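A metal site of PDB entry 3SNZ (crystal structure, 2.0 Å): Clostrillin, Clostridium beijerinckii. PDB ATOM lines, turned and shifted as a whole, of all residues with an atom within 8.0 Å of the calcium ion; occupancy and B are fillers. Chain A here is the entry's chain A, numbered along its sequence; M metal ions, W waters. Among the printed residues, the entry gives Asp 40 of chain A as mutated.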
ATOM      1  N   LEU A  28       7.181  12.355  -5.455  1.00  0.00           N
ATOM      2  CA  LEU A  28       6.651  11.752  -6.676  1.00  0.00           C
ATOM      3  C   LEU A  28       5.253  11.216  -6.453  1.00  0.00           C
ATOM      4  O   LEU A  28       4.357  11.465  -7.265  1.00  0.00           O
ATOM      5  CB  LEU A  28       7.564  10.647  -7.214  1.00  0.00           C
ATOM      6  CG  LEU A  28       7.132   9.923  -8.497  1.00  0.00           C
ATOM      7  CD1 LEU A  28       6.853  10.921  -9.608  1.00  0.00           C
ATOM      8  CD2 LEU A  28       8.194   8.879  -8.938  1.00  0.00           C
ATOM      9  N   ASN A  38       5.357  11.571 -13.659  1.00  0.00           N
ATOM     10  CA  ASN A  38       6.802  11.622 -13.598  1.00  0.00           C
ATOM     11  C   ASN A  38       7.403  12.148 -14.910  1.00  0.00           C
ATOM     12  O   ASN A  38       6.887  11.866 -15.995  1.00  0.00           O
ATOM     13  CB  ASN A  38       7.340  10.231 -13.319  1.00  0.00           C
ATOM     14  CG  ASN A  38       8.774  10.235 -12.841  1.00  0.00           C
ATOM     15  OD1 ASN A  38       9.273  11.247 -12.344  1.00  0.00           O
ATOM     16  ND2 ASN A  38       9.442   9.122 -12.990  1.00  0.00           N
ATOM     17  N   ASP A  39       8.485  12.915 -14.796  1.00  0.00           N
ATOM     18  CA  ASP A  39       9.315  13.320 -15.949  1.00  0.00           C
ATOM     19  C   ASP A  39       8.522  13.923 -17.106  1.00  0.00           C
ATOM     20  O   ASP A  39       8.730  13.546 -18.270  1.00  0.00           O
ATOM     21  CB  ASP A  39      10.126  12.123 -16.446  1.00  0.00           C
ATOM     22  CG  ASP A  39      11.107  11.617 -15.404  1.00  0.00           C
ATOM     23  OD1 ASP A  39      11.478  12.402 -14.513  1.00  0.00           O
ATOM     24  OD2 ASP A  39      11.516  10.433 -15.488  1.00  0.00           O
ATOM     25  N   ASP A  40       7.627  14.865 -16.809  1.00  0.00           N
ATOM     26  CA  ASP A  40       6.696  15.340 -17.829  1.00  0.00           C
ATOM     27  C   ASP A  40       6.546  16.863 -17.881  1.00  0.00           C
ATOM     28  O   ASP A  40       5.807  17.387 -18.723  1.00  0.00           O
ATOM     29  CB  ASP A  40       5.344  14.673 -17.625  1.00  0.00           C
ATOM     30  CG  ASP A  40       4.496  14.605 -18.892  1.00  0.00           C
ATOM     31  OD1 ASP A  40       5.027  14.703 -20.035  1.00  0.00           O
ATOM     32  OD2 ASP A  40       3.272  14.444 -18.743  1.00  0.00           O
ATOM     33  N   VAL A  54      12.790  22.345  -8.443  1.00  0.00           N
ATOM     34  CA  VAL A  54      12.486  21.135  -9.176  1.00  0.00           C
ATOM     35  C   VAL A  54      13.636  20.152  -9.007  1.00  0.00           C
ATOM     36  O   VAL A  54      14.797  20.502  -9.256  1.00  0.00           O
ATOM     37  CB  VAL A  54      12.310  21.466 -10.680  1.00  0.00           C
ATOM     38  CG1 VAL A  54      12.159  20.207 -11.522  1.00  0.00           C
ATOM     39  CG2 VAL A  54      11.109  22.419 -10.877  1.00  0.00           C
ATOM     40  N   TYR A  55      13.312  18.924  -8.598  1.00  0.00           N
ATOM     41  CA  TYR A  55      14.331  17.895  -8.370  1.00  0.00           C
ATOM     42  C   TYR A  55      14.205  16.756  -9.349  1.00  0.00           C
ATOM     43  O   TYR A  55      13.097  16.315  -9.665  1.00  0.00           O
ATOM     44  CB  TYR A  55      14.241  17.335  -6.954  1.00  0.00           C
ATOM     45  CG  TYR A  55      14.605  18.321  -5.884  1.00  0.00           C
ATOM     46  CD1 TYR A  55      15.930  18.441  -5.456  1.00  0.00           C
ATOM     47  CD2 TYR A  55      13.635  19.141  -5.298  1.00  0.00           C
ATOM     48  CE1 TYR A  55      16.279  19.351  -4.473  1.00  0.00           C
ATOM     49  CE2 TYR A  55      13.974  20.062  -4.309  1.00  0.00           C
ATOM     50  CZ  TYR A  55      15.303  20.151  -3.909  1.00  0.00           C
ATOM     51  OH  TYR A  55      15.638  21.053  -2.921  1.00  0.00           O
ATOM     52  N   GLU A  56      15.367  16.283  -9.818  1.00  0.00           N
ATOM     53  CA  GLU A  56      15.444  15.226 -10.821  1.00  0.00           C
ATOM     54  C   GLU A  56      15.002  13.886 -10.257  1.00  0.00           C
ATOM     55  O   GLU A  56      14.486  13.036 -10.986  1.00  0.00           O
ATOM     56  CB  GLU A  56      16.870  15.120 -11.402  1.00  0.00           C
ATOM     57  CG  GLU A  56      17.048  13.970 -12.404  1.00  0.00           C
ATOM     58  CD  GLU A  56      18.415  13.960 -13.088  1.00  0.00           C
ATOM     59  OE1 GLU A  56      19.453  14.103 -12.396  1.00  0.00           O
ATOM     60  OE2 GLU A  56      18.449  13.773 -14.320  1.00  0.00           O
ATOM     61  N   ASN A  57      15.209  13.675  -8.963  1.00  0.00           N
ATOM     62  CA  ASN A  57      14.873  12.405  -8.352  1.00  0.00           C
ATOM     63  C   ASN A  57      13.896  12.612  -7.195  1.00  0.00           C
ATOM     64  O   ASN A  57      13.606  13.755  -6.795  1.00  0.00           O
ATOM     65  CB  ASN A  57      16.142  11.667  -7.883  1.00  0.00           C
ATOM     66  CG  ASN A  57      17.042  11.241  -9.046  1.00  0.00           C
ATOM     67  OD1 ASN A  57      16.576  10.723 -10.054  1.00  0.00           O
ATOM     68  ND2 ASN A  57      18.332  11.455  -8.894  1.00  0.00           N
ATOM     69  N   ASP A  58      13.409  11.506  -6.642  1.00  0.00           N
ATOM     70  CA  ASP A  58      12.371  11.565  -5.629  1.00  0.00           C
ATOM     71  C   ASP A  58      12.925  12.028  -4.294  1.00  0.00           C
ATOM     72  O   ASP A  58      14.148  11.958  -4.043  1.00  0.00           O
ATOM     73  CB  ASP A  58      11.663  10.216  -5.478  1.00  0.00           C
ATOM     74  CG  ASP A  58      10.281  10.332  -4.838  1.00  0.00           C
ATOM     75  OD1 ASP A  58       9.791  11.469  -4.600  1.00  0.00           O
ATOM     76  OD2 ASP A  58       9.676   9.276  -4.569  1.00  0.00           O
ATOM     77  N   THR A  61      15.911  14.989  -4.132  1.00  0.00           N
ATOM     78  CA  THR A  61      17.307  14.586  -4.353  1.00  0.00           C
ATOM     79  C   THR A  61      17.617  14.593  -5.844  1.00  0.00           C
ATOM     80  O   THR A  61      16.726  14.852  -6.665  1.00  0.00           O
ATOM     81  CB  THR A  61      17.661  13.196  -3.749  1.00  0.00           C
ATOM     82  OG1 THR A  61      16.844  12.169  -4.336  1.00  0.00           O
ATOM     83  CG2 THR A  61      17.521  13.174  -2.224  1.00  0.00           C
ATOM     84  N   THR A  63      19.707  16.273  -9.152  1.00  0.00           N
ATOM     85  CA  THR A  63      19.886  17.645  -9.615  1.00  0.00           C
ATOM     86  C   THR A  63      18.662  18.511  -9.333  1.00  0.00           C
ATOM     87  O   THR A  63      17.518  18.053  -9.457  1.00  0.00           O
ATOM     88  CB  THR A  63      20.196  17.693 -11.140  1.00  0.00           C
ATOM     89  OG1 THR A  63      21.368  16.928 -11.405  1.00  0.00           O
ATOM     90  CG2 THR A  63      20.423  19.126 -11.610  1.00  0.00           C
ATOM     91  N   TRP A  65      16.778  22.228 -10.118  1.00  0.00           N
ATOM     92  CA  TRP A  65      16.638  23.466 -10.900  1.00  0.00           C
ATOM     93  C   TRP A  65      15.695  24.420 -10.171  1.00  0.00           C
ATOM     94  O   TRP A  65      14.678  23.994  -9.636  1.00  0.00           O
ATOM     95  CB  TRP A  65      16.107  23.174 -12.311  1.00  0.00           C
ATOM     96  CG  TRP A  65      16.993  22.253 -13.096  1.00  0.00           C
ATOM     97  CD1 TRP A  65      18.083  22.597 -13.833  1.00  0.00           C
ATOM     98  CD2 TRP A  65      16.872  20.820 -13.197  1.00  0.00           C
ATOM     99  NE1 TRP A  65      18.652  21.481 -14.396  1.00  0.00           N
ATOM    100  CE2 TRP A  65      17.923  20.377 -14.033  1.00  0.00           C
ATOM    101  CE3 TRP A  65      15.966  19.882 -12.687  1.00  0.00           C
ATOM    102  CZ2 TRP A  65      18.104  19.020 -14.355  1.00  0.00           C
ATOM    103  CZ3 TRP A  65      16.136  18.537 -13.003  1.00  0.00           C
ATOM    104  CH2 TRP A  65      17.202  18.122 -13.834  1.00  0.00           C
ATOM    105  N   ALA A  78      16.869  20.276 -18.190  1.00  0.00           N
ATOM    106  CA  ALA A  78      15.821  20.163 -17.160  1.00  0.00           C
ATOM    107  C   ALA A  78      14.481  19.630 -17.688  1.00  0.00           C
ATOM    108  O   ALA A  78      13.624  19.238 -16.901  1.00  0.00           O
ATOM    109  CB  ALA A  78      15.605  21.521 -16.475  1.00  0.00           C
ATOM    110  N   ASN A  79      14.303  19.631 -19.002  1.00  0.00           N
ATOM    111  CA  ASN A  79      13.020  19.231 -19.602  1.00  0.00           C
ATOM    112  C   ASN A  79      12.641  17.791 -19.277  1.00  0.00           C
ATOM    113  O   ASN A  79      13.488  16.895 -19.348  1.00  0.00           O
ATOM    114  CB  ASN A  79      13.030  19.422 -21.123  1.00  0.00           C
ATOM    115  CG  ASN A  79      11.656  19.285 -21.742  1.00  0.00           C
ATOM    116  OD1 ASN A  79      10.642  19.427 -21.046  1.00  0.00           O
ATOM    117  ND2 ASN A  79      11.601  19.006 -23.045  1.00  0.00           N
ATOM    118  N   ASP A  80      11.375  17.572 -18.915  1.00  0.00           N
ATOM    119  CA  ASP A  80      10.853  16.223 -18.597  1.00  0.00           C
ATOM    120  C   ASP A  80      11.685  15.471 -17.534  1.00  0.00           C
ATOM    121  O   ASP A  80      11.910  14.264 -17.666  1.00  0.00           O
ATOM    122  CB  ASP A  80      10.720  15.397 -19.888  1.00  0.00           C
ATOM    123  CG  ASP A  80       9.651  15.960 -20.816  1.00  0.00           C
ATOM    124  OD1 ASP A  80       8.802  16.716 -20.319  1.00  0.00           O
ATOM    125  OD2 ASP A  80       9.676  15.653 -22.034  1.00  0.00           O
ATOM    126  N   LYS A  81      12.116  16.189 -16.498  1.00  0.00           N
ATOM    127  CA  LYS A  81      12.945  15.622 -15.436  1.00  0.00           C
ATOM    128  C   LYS A  81      12.342  15.707 -14.042  1.00  0.00           C
ATOM    129  O   LYS A  81      12.875  15.121 -13.104  1.00  0.00           O
ATOM    130  CB  LYS A  81      14.342  16.265 -15.407  1.00  0.00           C
ATOM    131  CG  LYS A  81      15.214  15.989 -16.643  1.00  0.00           C
ATOM    132  CD  LYS A  81      15.533  14.509 -16.798  1.00  0.00           C
ATOM    133  CE  LYS A  81      16.934  14.285 -17.350  1.00  0.00           C
ATOM    134  NZ  LYS A  81      17.164  15.069 -18.585  1.00  0.00           N
ATOM    135  N   MET A  82      11.223  16.422 -13.883  1.00  0.00           N
ATOM    136  CA  MET A  82      10.661  16.602 -12.542  1.00  0.00           C
ATOM    137  C   MET A  82      10.086  15.330 -11.938  1.00  0.00           C
ATOM    138  O   MET A  82       9.157  14.734 -12.486  1.00  0.00           O
ATOM    139  CB  MET A  82       9.622  17.722 -12.505  1.00  0.00           C
ATOM    140  CG  MET A  82       9.056  17.932 -11.082  1.00  0.00           C
ATOM    141  SD  MET A  82       7.746  19.128 -11.068  1.00  0.00           S
ATOM    142  CE  MET A  82       8.685  20.619 -11.008  1.00  0.00           C
ATOM    143  N   THR A  83      10.654  14.916 -10.803  1.00  0.00           N
ATOM    144  CA  THR A  83      10.174  13.774 -10.041  1.00  0.00           C
ATOM    145  C   THR A  83       9.722  14.185  -8.630  1.00  0.00           C
ATOM    146  O   THR A  83       8.852  13.555  -8.048  1.00  0.00           O
ATOM    147  CB  THR A  83      11.251  12.655  -9.978  1.00  0.00           C
ATOM    148  OG1 THR A  83      11.472  12.146 -11.301  1.00  0.00           O
ATOM    149  CG2 THR A  83      10.832  11.508  -9.095  1.00  0.00           C
ATOM    150  N   SER A  84      10.325  15.235  -8.072  1.00  0.00           N
ATOM    151  CA  SER A  84       9.809  15.858  -6.859  1.00  0.00           C
ATOM    152  C   SER A  84      10.034  17.365  -6.925  1.00  0.00           C
ATOM    153  O   SER A  84      10.799  17.828  -7.774  1.00  0.00           O
ATOM    154  CB  SER A  84      10.426  15.238  -5.597  1.00  0.00           C
ATOM    155  OG  SER A  84      11.832  15.429  -5.527  1.00  0.00           O
HETATM  156 CA    CA M   1      13.170  12.596 -12.873  1.00  0.00          CA
HETATM  157  O   HOH W   1      13.508   9.851 -13.805  1.00  0.00           O
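Four residues have an atom within 4 Å of the calcium ion: Asp 39, Glu 56, Lys 81 and Thr 83.
The calcium ion is bound by the backbone carbonyl oxygen (O) of Glu 56.
The calcium ion is bound by the side-chain hydroxyl (OG1) of Thr 83 (2.4 Å).
The calcium ion is bound by the side-chain carboxylate (OD1) of Asp 39.
O of Lys 81 is bound to the calcium ion (2.6 Å).
The calcium ion has four donor atoms within binding distance.
Slightly farther from the calcium ion lies water W1 (2.9 Å).
O of Thr 83 lies close to N of Leu 28 (3.3 Å).
The backbone carbonyl oxygen of Tyr 55 sits at hydrogen-bond distance from the backbone NH of Thr 83 (3.0 Å).
N of Glu 56 sits at hydrogen-bond distance from O of Thr 63 (2.8 Å).
OD1 of Asp 39 lies close to OD1 of Asn 38.
The side-chain hydroxyl of Thr 83 lies close to the side-chain amide oxygen of Asn 38.
The backbone NH (N) of Asp 39 sits at hydrogen-bond distance from the backbone carbonyl oxygen (O) of Met 82 (3.0 Å).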
